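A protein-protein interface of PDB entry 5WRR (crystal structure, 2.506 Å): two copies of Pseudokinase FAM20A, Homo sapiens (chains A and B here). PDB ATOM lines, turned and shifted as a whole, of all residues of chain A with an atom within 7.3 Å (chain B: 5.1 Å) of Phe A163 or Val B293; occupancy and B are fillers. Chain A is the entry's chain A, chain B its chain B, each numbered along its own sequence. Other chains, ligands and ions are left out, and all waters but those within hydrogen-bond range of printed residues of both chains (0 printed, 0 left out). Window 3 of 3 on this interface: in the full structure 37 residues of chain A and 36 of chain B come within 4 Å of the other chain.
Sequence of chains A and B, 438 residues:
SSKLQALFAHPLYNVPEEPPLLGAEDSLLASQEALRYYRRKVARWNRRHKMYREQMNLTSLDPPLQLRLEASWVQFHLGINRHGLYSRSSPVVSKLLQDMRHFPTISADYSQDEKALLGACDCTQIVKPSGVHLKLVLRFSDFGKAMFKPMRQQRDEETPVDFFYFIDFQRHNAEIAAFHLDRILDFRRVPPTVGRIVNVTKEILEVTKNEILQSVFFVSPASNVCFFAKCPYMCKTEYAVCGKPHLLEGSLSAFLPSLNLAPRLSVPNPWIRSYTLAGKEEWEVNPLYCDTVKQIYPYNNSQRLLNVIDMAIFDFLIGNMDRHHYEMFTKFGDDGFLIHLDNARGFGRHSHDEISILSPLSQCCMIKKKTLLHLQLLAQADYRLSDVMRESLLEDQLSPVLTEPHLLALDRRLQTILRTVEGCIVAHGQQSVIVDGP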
ATOM      1  N   ASP A 156     -13.085   2.662 -14.557  1.00  0.00           N
ATOM      2  CA  ASP A 156     -12.664   3.181 -13.260  1.00  0.00           C
ATOM      3  C   ASP A 156     -13.591   2.767 -12.125  1.00  0.00           C
ATOM      4  O   ASP A 156     -13.210   2.915 -10.960  1.00  0.00           O
ATOM      5  CB  ASP A 156     -12.533   4.707 -13.301  1.00  0.00           C
ATOM      6  CG  ASP A 156     -13.798   5.395 -13.758  1.00  0.00           C
ATOM      7  OD1 ASP A 156     -14.282   5.075 -14.863  1.00  0.00           O
ATOM      8  OD2 ASP A 156     -14.305   6.261 -13.013  1.00  0.00           O
ATOM      9  N   THR A 159     -11.748   0.244 -10.482  1.00  0.00           N
ATOM     10  CA  THR A 159     -10.521   0.756  -9.870  1.00  0.00           C
ATOM     11  C   THR A 159     -10.889   1.956  -9.006  1.00  0.00           C
ATOM     12  O   THR A 159     -10.651   3.111  -9.388  1.00  0.00           O
ATOM     13  CB  THR A 159      -9.488   1.130 -10.934  1.00  0.00           C
ATOM     14  OG1 THR A 159      -9.964   2.245 -11.699  1.00  0.00           O
ATOM     15  CG2 THR A 159      -9.260  -0.039 -11.874  1.00  0.00           C
ATOM     16  N   PRO A 160     -11.465   1.717  -7.823  1.00  0.00           N
ATOM     17  CA  PRO A 160     -12.015   2.832  -7.031  1.00  0.00           C
ATOM     18  C   PRO A 160     -10.995   3.892  -6.660  1.00  0.00           C
ATOM     19  O   PRO A 160     -11.366   5.059  -6.481  1.00  0.00           O
ATOM     20  CB  PRO A 160     -12.566   2.130  -5.780  1.00  0.00           C
ATOM     21  CG  PRO A 160     -12.772   0.710  -6.192  1.00  0.00           C
ATOM     22  CD  PRO A 160     -11.686   0.413  -7.176  1.00  0.00           C
ATOM     23  N   VAL A 161      -9.716   3.530  -6.552  1.00  0.00           N
ATOM     24  CA  VAL A 161      -8.701   4.500  -6.157  1.00  0.00           C
ATOM     25  C   VAL A 161      -8.278   5.398  -7.318  1.00  0.00           C
ATOM     26  O   VAL A 161      -7.867   6.543  -7.087  1.00  0.00           O
ATOM     27  CB  VAL A 161      -7.503   3.752  -5.541  1.00  0.00           C
ATOM     28  CG1 VAL A 161      -6.174   4.232  -6.120  1.00  0.00           C
ATOM     29  CG2 VAL A 161      -7.516   3.889  -4.024  1.00  0.00           C
ATOM     30  N   ASP A 162      -8.424   4.939  -8.558  1.00  0.00           N
ATOM     31  CA  ASP A 162      -7.972   5.721  -9.701  1.00  0.00           C
ATOM     32  C   ASP A 162      -8.879   6.922  -9.944  1.00  0.00           C
ATOM     33  O   ASP A 162     -10.108   6.815  -9.909  1.00  0.00           O
ATOM     34  CB  ASP A 162      -7.928   4.849 -10.958  1.00  0.00           C
ATOM     35  CG  ASP A 162      -6.829   3.806 -10.908  1.00  0.00           C
ATOM     36  OD1 ASP A 162      -6.162   3.689  -9.858  1.00  0.00           O
ATOM     37  OD2 ASP A 162      -6.634   3.102 -11.921  1.00  0.00           O
ATOM     38  N   PHE A 163      -8.260   8.073 -10.195  1.00  0.00           N
ATOM     39  CA  PHE A 163      -8.979   9.280 -10.582  1.00  0.00           C
ATOM     40  C   PHE A 163      -9.114   9.312 -12.101  1.00  0.00           C
ATOM     41  O   PHE A 163      -8.117   9.180 -12.818  1.00  0.00           O
ATOM     42  CB  PHE A 163      -8.256  10.528 -10.071  1.00  0.00           C
ATOM     43  CG  PHE A 163      -8.972  11.810 -10.382  1.00  0.00           C
ATOM     44  CD1 PHE A 163     -10.212  12.079  -9.830  1.00  0.00           C
ATOM     45  CD2 PHE A 163      -8.401  12.746 -11.229  1.00  0.00           C
ATOM     46  CE1 PHE A 163     -10.872  13.262 -10.114  1.00  0.00           C
ATOM     47  CE2 PHE A 163      -9.055  13.929 -11.519  1.00  0.00           C
ATOM     48  CZ  PHE A 163     -10.291  14.189 -10.961  1.00  0.00           C
ATOM     49  N   PHE A 164     -10.352   9.493 -12.576  1.00  0.00           N
ATOM     50  CA  PHE A 164     -10.688   9.307 -13.989  1.00  0.00           C
ATOM     51  C   PHE A 164      -9.720  10.024 -14.927  1.00  0.00           C
ATOM     52  O   PHE A 164      -9.163   9.414 -15.847  1.00  0.00           O
ATOM     53  CB  PHE A 164     -12.121   9.783 -14.241  1.00  0.00           C
ATOM     54  CG  PHE A 164     -12.563   9.654 -15.671  1.00  0.00           C
ATOM     55  CD1 PHE A 164     -12.948   8.426 -16.186  1.00  0.00           C
ATOM     56  CD2 PHE A 164     -12.603  10.764 -16.500  1.00  0.00           C
ATOM     57  CE1 PHE A 164     -13.358   8.308 -17.503  1.00  0.00           C
ATOM     58  CE2 PHE A 164     -13.011  10.652 -17.815  1.00  0.00           C
ATOM     59  CZ  PHE A 164     -13.388   9.424 -18.318  1.00  0.00           C
ATOM     60  N   TYR A 165      -9.513  11.322 -14.717  1.00  0.00           N
ATOM     61  CA  TYR A 165      -8.734  12.134 -15.643  1.00  0.00           C
ATOM     62  C   TYR A 165      -7.231  11.890 -15.542  1.00  0.00           C
ATOM     63  O   TYR A 165      -6.461  12.586 -16.214  1.00  0.00           O
ATOM     64  CB  TYR A 165      -9.047  13.616 -15.426  1.00  0.00           C
ATOM     65  CG  TYR A 165     -10.489  13.950 -15.733  1.00  0.00           C
ATOM     66  CD1 TYR A 165     -10.919  14.115 -17.043  1.00  0.00           C
ATOM     67  CD2 TYR A 165     -11.425  14.072 -14.717  1.00  0.00           C
ATOM     68  CE1 TYR A 165     -12.240  14.410 -17.330  1.00  0.00           C
ATOM     69  CE2 TYR A 165     -12.746  14.364 -14.993  1.00  0.00           C
ATOM     70  CZ  TYR A 165     -13.149  14.532 -16.301  1.00  0.00           C
ATOM     71  OH  TYR A 165     -14.465  14.824 -16.576  1.00  0.00           O
ATOM     72  N   PHE A 166      -6.798  10.927 -14.731  1.00  0.00           N
ATOM     73  CA  PHE A 166      -5.399  10.530 -14.673  1.00  0.00           C
ATOM     74  C   PHE A 166      -5.168   9.141 -15.249  1.00  0.00           C
ATOM     75  O   PHE A 166      -4.018   8.696 -15.319  1.00  0.00           O
ATOM     76  CB  PHE A 166      -4.880  10.569 -13.228  1.00  0.00           C
ATOM     77  CG  PHE A 166      -4.822  11.946 -12.629  1.00  0.00           C
ATOM     78  CD1 PHE A 166      -4.964  13.079 -13.416  1.00  0.00           C
ATOM     79  CD2 PHE A 166      -4.616  12.107 -11.267  1.00  0.00           C
ATOM     80  CE1 PHE A 166      -4.910  14.343 -12.852  1.00  0.00           C
ATOM     81  CE2 PHE A 166      -4.558  13.364 -10.701  1.00  0.00           C
ATOM     82  CZ  PHE A 166      -4.705  14.484 -11.494  1.00  0.00           C
ATOM     83  N   ILE A 167      -6.227   8.450 -15.664  1.00  0.00           N
ATOM     84  CA  ILE A 167      -6.115   7.078 -16.142  1.00  0.00           C
ATOM     85  C   ILE A 167      -5.511   7.074 -17.539  1.00  0.00           C
ATOM     86  O   ILE A 167      -5.900   7.868 -18.403  1.00  0.00           O
ATOM     87  CB  ILE A 167      -7.493   6.392 -16.125  1.00  0.00           C
ATOM     88  CG1 ILE A 167      -8.001   6.252 -14.692  1.00  0.00           C
ATOM     89  CG2 ILE A 167      -7.428   5.024 -16.794  1.00  0.00           C
ATOM     90  CD1 ILE A 167      -9.379   5.651 -14.601  1.00  0.00           C
ATOM     91  N   ASP A 168      -4.553   6.170 -17.758  1.00  0.00           N
ATOM     92  CA  ASP A 168      -3.858   6.037 -19.041  1.00  0.00           C
ATOM     93  C   ASP A 168      -4.658   5.132 -19.984  1.00  0.00           C
ATOM     94  O   ASP A 168      -4.244   4.033 -20.357  1.00  0.00           O
ATOM     95  CB  ASP A 168      -2.441   5.521 -18.821  1.00  0.00           C
ATOM     96  CG  ASP A 168      -2.398   4.255 -17.976  1.00  0.00           C
ATOM     97  OD1 ASP A 168      -3.469   3.809 -17.514  1.00  0.00           O
ATOM     98  OD2 ASP A 168      -1.292   3.712 -17.767  1.00  0.00           O
ATOM     99  N   PHE A 169      -5.842   5.619 -20.366  1.00  0.00           N
ATOM    100  CA  PHE A 169      -6.677   4.875 -21.306  1.00  0.00           C
ATOM    101  C   PHE A 169      -5.990   4.731 -22.662  1.00  0.00           C
ATOM    102  O   PHE A 169      -6.079   3.676 -23.303  1.00  0.00           O
ATOM    103  CB  PHE A 169      -8.032   5.562 -21.465  1.00  0.00           C
ATOM    104  CG  PHE A 169      -8.981   5.306 -20.334  1.00  0.00           C
ATOM    105  CD1 PHE A 169      -9.277   4.012 -19.939  1.00  0.00           C
ATOM    106  CD2 PHE A 169      -9.577   6.361 -19.662  1.00  0.00           C
ATOM    107  CE1 PHE A 169     -10.154   3.773 -18.893  1.00  0.00           C
ATOM    108  CE2 PHE A 169     -10.453   6.131 -18.617  1.00  0.00           C
ATOM    109  CZ  PHE A 169     -10.743   4.834 -18.231  1.00  0.00           C
ATOM    110  N   PRO B 268      -4.712   9.306  -5.588  1.00  0.00           N
ATOM    111  CA  PRO B 268      -4.088  10.436  -6.288  1.00  0.00           C
ATOM    112  C   PRO B 268      -4.791  11.750  -5.989  1.00  0.00           C
ATOM    113  O   PRO B 268      -6.015  11.812  -5.850  1.00  0.00           O
ATOM    114  CB  PRO B 268      -4.217  10.053  -7.766  1.00  0.00           C
ATOM    115  CG  PRO B 268      -5.355   9.084  -7.808  1.00  0.00           C
ATOM    116  CD  PRO B 268      -5.294   8.325  -6.521  1.00  0.00           C
ATOM    117  N   PRO B 270      -6.246  15.021  -7.119  1.00  0.00           N
ATOM    118  CA  PRO B 270      -6.759  15.573  -8.385  1.00  0.00           C
ATOM    119  C   PRO B 270      -6.236  16.963  -8.715  1.00  0.00           C
ATOM    120  O   PRO B 270      -6.409  17.408  -9.857  1.00  0.00           O
ATOM    121  CB  PRO B 270      -8.281  15.594  -8.172  1.00  0.00           C
ATOM    122  CG  PRO B 270      -8.531  14.630  -7.054  1.00  0.00           C
ATOM    123  CD  PRO B 270      -7.329  14.721  -6.168  1.00  0.00           C
ATOM    124  N   TRP B 271      -5.613  17.662  -7.766  1.00  0.00           N
ATOM    125  CA  TRP B 271      -5.081  19.000  -7.993  1.00  0.00           C
ATOM    126  C   TRP B 271      -3.558  19.046  -7.924  1.00  0.00           C
ATOM    127  O   TRP B 271      -2.985  20.119  -7.709  1.00  0.00           O
ATOM    128  CB  TRP B 271      -5.688  19.994  -7.000  1.00  0.00           C
ATOM    129  CG  TRP B 271      -7.114  20.352  -7.296  1.00  0.00           C
ATOM    130  CD1 TRP B 271      -7.555  21.349  -8.119  1.00  0.00           C
ATOM    131  CD2 TRP B 271      -8.288  19.719  -6.769  1.00  0.00           C
ATOM    132  NE1 TRP B 271      -8.929  21.376  -8.139  1.00  0.00           N
ATOM    133  CE2 TRP B 271      -9.404  20.386  -7.318  1.00  0.00           C
ATOM    134  CE3 TRP B 271      -8.504  18.656  -5.887  1.00  0.00           C
ATOM    135  CZ2 TRP B 271     -10.714  20.024  -7.012  1.00  0.00           C
ATOM    136  CZ3 TRP B 271      -9.809  18.297  -5.586  1.00  0.00           C
ATOM    137  CH2 TRP B 271     -10.896  18.979  -6.148  1.00  0.00           C
ATOM    138  N   LEU B 288     -15.182  25.061 -12.947  1.00  0.00           N
ATOM    139  CA  LEU B 288     -15.680  23.939 -13.742  1.00  0.00           C
ATOM    140  C   LEU B 288     -14.991  22.632 -13.372  1.00  0.00           C
ATOM    141  O   LEU B 288     -15.638  21.578 -13.314  1.00  0.00           O
ATOM    142  CB  LEU B 288     -15.514  24.226 -15.235  1.00  0.00           C
ATOM    143  CG  LEU B 288     -16.742  24.760 -15.977  1.00  0.00           C
ATOM    144  CD1 LEU B 288     -17.684  23.616 -16.315  1.00  0.00           C
ATOM    145  CD2 LEU B 288     -17.466  25.822 -15.160  1.00  0.00           C
ATOM    146  N   TYR B 289     -13.676  22.670 -13.138  1.00  0.00           N
ATOM    147  CA  TYR B 289     -12.960  21.448 -12.782  1.00  0.00           C
ATOM    148  C   TYR B 289     -13.507  20.851 -11.491  1.00  0.00           C
ATOM    149  O   TYR B 289     -13.834  19.658 -11.436  1.00  0.00           O
ATOM    150  CB  TYR B 289     -11.462  21.721 -12.661  1.00  0.00           C
ATOM    151  CG  TYR B 289     -10.644  20.473 -12.395  1.00  0.00           C
ATOM    152  CD1 TYR B 289     -10.593  19.441 -13.324  1.00  0.00           C
ATOM    153  CD2 TYR B 289      -9.921  20.328 -11.219  1.00  0.00           C
ATOM    154  CE1 TYR B 289      -9.848  18.299 -13.086  1.00  0.00           C
ATOM    155  CE2 TYR B 289      -9.171  19.192 -10.974  1.00  0.00           C
ATOM    156  CZ  TYR B 289      -9.138  18.180 -11.910  1.00  0.00           C
ATOM    157  OH  TYR B 289      -8.392  17.048 -11.666  1.00  0.00           O
ATOM    158  N   CYS B 290     -13.628  21.666 -10.439  1.00  0.00           N
ATOM    159  CA  CYS B 290     -14.189  21.145  -9.198  1.00  0.00           C
ATOM    160  C   CYS B 290     -15.668  20.815  -9.352  1.00  0.00           C
ATOM    161  O   CYS B 290     -16.159  19.879  -8.711  1.00  0.00           O
ATOM    162  CB  CYS B 290     -13.980  22.131  -8.046  1.00  0.00           C
ATOM    163  SG  CYS B 290     -14.569  21.461  -6.466  1.00  0.00           S
ATOM    164  N   ASP B 291     -16.388  21.555 -10.202  1.00  0.00           N
ATOM    165  CA  ASP B 291     -17.769  21.190 -10.511  1.00  0.00           C
ATOM    166  C   ASP B 291     -17.853  19.770 -11.060  1.00  0.00           C
ATOM    167  O   ASP B 291     -18.817  19.046 -10.787  1.00  0.00           O
ATOM    168  CB  ASP B 291     -18.370  22.182 -11.506  1.00  0.00           C
ATOM    169  CG  ASP B 291     -18.649  23.535 -10.886  1.00  0.00           C
ATOM    170  OD1 ASP B 291     -18.990  23.582  -9.685  1.00  0.00           O
ATOM    171  OD2 ASP B 291     -18.527  24.551 -11.602  1.00  0.00           O
ATOM    172  N   THR B 292     -16.850  19.357 -11.839  1.00  0.00           N
ATOM    173  CA  THR B 292     -16.817  17.989 -12.346  1.00  0.00           C
ATOM    174  C   THR B 292     -16.354  17.009 -11.275  1.00  0.00           C
ATOM    175  O   THR B 292     -16.933  15.927 -11.130  1.00  0.00           O
ATOM    176  CB  THR B 292     -15.907  17.901 -13.570  1.00  0.00           C
ATOM    177  OG1 THR B 292     -16.329  18.856 -14.551  1.00  0.00           O
ATOM    178  CG2 THR B 292     -15.961  16.505 -14.169  1.00  0.00           C
ATOM    179  N   VAL B 293     -15.314  17.370 -10.518  1.00  0.00           N
ATOM    180  CA  VAL B 293     -14.809  16.487  -9.468  1.00  0.00           C
ATOM    181  C   VAL B 293     -15.885  16.239  -8.419  1.00  0.00           C
ATOM    182  O   VAL B 293     -15.990  15.137  -7.866  1.00  0.00           O
ATOM    183  CB  VAL B 293     -13.526  17.070  -8.846  1.00  0.00           C
ATOM    184  CG1 VAL B 293     -13.039  16.193  -7.702  1.00  0.00           C
ATOM    185  CG2 VAL B 293     -12.444  17.205  -9.900  1.00  0.00           C
ATOM    186  N   LYS B 294     -16.706  17.256  -8.130  1.00  0.00           N
ATOM    187  CA  LYS B 294     -17.820  17.083  -7.202  1.00  0.00           C
ATOM    188  C   LYS B 294     -18.773  15.979  -7.641  1.00  0.00           C
ATOM    189  O   LYS B 294     -19.488  15.423  -6.801  1.00  0.00           O
ATOM    190  CB  LYS B 294     -18.598  18.392  -7.046  1.00  0.00           C
ATOM    191  CG  LYS B 294     -17.928  19.438  -6.163  1.00  0.00           C
ATOM    192  CD  LYS B 294     -18.713  20.744  -6.178  1.00  0.00           C
ATOM    193  CE  LYS B 294     -17.946  21.869  -5.506  1.00  0.00           C
ATOM    194  NZ  LYS B 294     -18.831  23.004  -5.126  1.00  0.00           N
ATOM    195  N   GLN B 295     -18.810  15.658  -8.932  1.00  0.00           N
ATOM    196  CA  GLN B 295     -19.664  14.604  -9.457  1.00  0.00           C
ATOM    197  C   GLN B 295     -18.928  13.281  -9.626  1.00  0.00           C
ATOM    198  O   GLN B 295     -19.491  12.341 -10.196  1.00  0.00           O
ATOM    199  CB  GLN B 295     -20.270  15.036 -10.793  1.00  0.00           C
ATOM    200  CG  GLN B 295     -21.070  16.325 -10.725  1.00  0.00           C
ATOM    201  CD  GLN B 295     -21.630  16.731 -12.071  1.00  0.00           C
ATOM    202  OE1 GLN B 295     -22.765  16.398 -12.412  1.00  0.00           O
ATOM    203  NE2 GLN B 295     -20.833  17.455 -12.849  1.00  0.00           N
ATOM    204  N   ILE B 296     -17.693  13.185  -9.144  1.00  0.00           N
ATOM    205  CA  ILE B 296     -16.868  11.992  -9.302  1.00  0.00           C
ATOM    206  C   ILE B 296     -16.647  11.374  -7.928  1.00  0.00           C
ATOM    207  O   ILE B 296     -16.133  12.035  -7.017  1.00  0.00           O
ATOM    208  CB  ILE B 296     -15.529  12.315  -9.981  1.00  0.00           C
ATOM    209  CG1 ILE B 296     -15.759  12.821 -11.407  1.00  0.00           C
ATOM    210  CG2 ILE B 296     -14.624  11.093  -9.985  1.00  0.00           C
ATOM    211  CD1 ILE B 296     -14.483  13.149 -12.146  1.00  0.00           C
ATOM    212  N   TYR B 299     -15.523  11.984  -4.302  1.00  0.00           N
ATOM    213  CA  TYR B 299     -15.638  13.399  -3.977  1.00  0.00           C
ATOM    214  C   TYR B 299     -17.072  13.909  -4.037  1.00  0.00           C
ATOM    215  O   TYR B 299     -17.291  15.114  -3.883  1.00  0.00           O
ATOM    216  CB  TYR B 299     -14.736  14.222  -4.899  1.00  0.00           C
ATOM    217  CG  TYR B 299     -13.286  13.799  -4.818  1.00  0.00           C
ATOM    218  CD1 TYR B 299     -12.478  14.223  -3.769  1.00  0.00           C
ATOM    219  CD2 TYR B 299     -12.728  12.964  -5.779  1.00  0.00           C
ATOM    220  CE1 TYR B 299     -11.153  13.833  -3.683  1.00  0.00           C
ATOM    221  CE2 TYR B 299     -11.402  12.571  -5.701  1.00  0.00           C
ATOM    222  CZ  TYR B 299     -10.620  13.008  -4.651  1.00  0.00           C
ATOM    223  OH  TYR B 299      -9.301  12.620  -4.567  1.00  0.00           O
ATOM    224  N   ASN B 300     -18.055  13.035  -4.259  1.00  0.00           N
ATOM    225  CA  ASN B 300     -19.433  13.506  -4.231  1.00  0.00           C
ATOM    226  C   ASN B 300     -19.931  13.734  -2.819  1.00  0.00           C
ATOM    227  O   ASN B 300     -20.845  14.539  -2.621  1.00  0.00           O
ATOM    228  CB  ASN B 300     -20.384  12.513  -4.878  1.00  0.00           C
ATOM    229  CG  ASN B 300     -20.313  11.143  -4.247  1.00  0.00           C
ATOM    230  OD1 ASN B 300     -19.250  10.521  -4.185  1.00  0.00           O
ATOM    231  ND2 ASN B 300     -21.446  10.684  -3.725  1.00  0.00           N
ATOM    232  N   LEU B 305     -14.229  15.981   0.038  1.00  0.00           N
ATOM    233  CA  LEU B 305     -13.746  17.198  -0.610  1.00  0.00           C
ATOM    234  C   LEU B 305     -13.283  18.223   0.417  1.00  0.00           C
ATOM    235  O   LEU B 305     -12.300  18.939   0.189  1.00  0.00           O
ATOM    236  CB  LEU B 305     -14.829  17.787  -1.510  1.00  0.00           C
ATOM    237  CG  LEU B 305     -14.362  18.918  -2.430  1.00  0.00           C
ATOM    238  CD1 LEU B 305     -13.194  18.458  -3.290  1.00  0.00           C
ATOM    239  CD2 LEU B 305     -15.507  19.422  -3.296  1.00  0.00           C
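The backbone carbonyl oxygen (O) of Pro B270 lies within hydrogen-bond range of the side-chain hydroxyl (OH) of Tyr B289 (2.7 Å). The backbone carbonyl oxygen (O) of Leu B288 sits at hydrogen-bond distance from the side-chain hydroxyl (OG1) of Thr B292, 3.1 Å away.
Val A161 touches Pro B268. Phe A163 touches Pro B268. Phe A163 touches Pro B270 (CZ to CB, 3.7 Å). OH of Tyr B289 touches CE2 of Phe A163 (3.2 Å). Phe A163 touches Val B293. Thr B292 touches Tyr A165 (CG2 to OH, 3.3 Å). Tyr A165 touches Ile B296. Pro B270 touches Phe A166.
Of chain B, only Pro B268, Pro B270, Tyr B289 and Val B293 come within 4 Å of Phe A163. Of the printed residues of chain B, Tyr A165 touches Thr B292 and Ile B296. Of the printed residues of chain A, Pro B270 touches Phe A163 and Phe A166. Of the printed residues of chain A, Tyr B289 touches Phe A163. Of chain A, only Phe A163 comes within 4 Å of Val B293. Of the printed residues of chain A, Ile B296 touches Tyr A165. The nearest residue of chain B that does not touch Phe A163 is Ile B296 (4.1 Å). The nearest residue of chain A that does not touch Val B293 is Tyr A165 (5.8 Å). The nearest printed residue of chain A that does not touch Thr B292 is Phe A163 (6.7 Å).
Hydrophobic or aromatic side chains of chain B within 4 Å of the printed part of chain A: Pro B268, Pro B270, Tyr B289, Val B293 and Ile B296. Of the 12 printed residues of chain A, 4 touch a printed residue of chain B. Hydrophobic or aromatic side chains of chain A within 4 Å of the printed part of chain B: Phe A163, Tyr A165 and Phe A166.
No position is printed for both chains.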
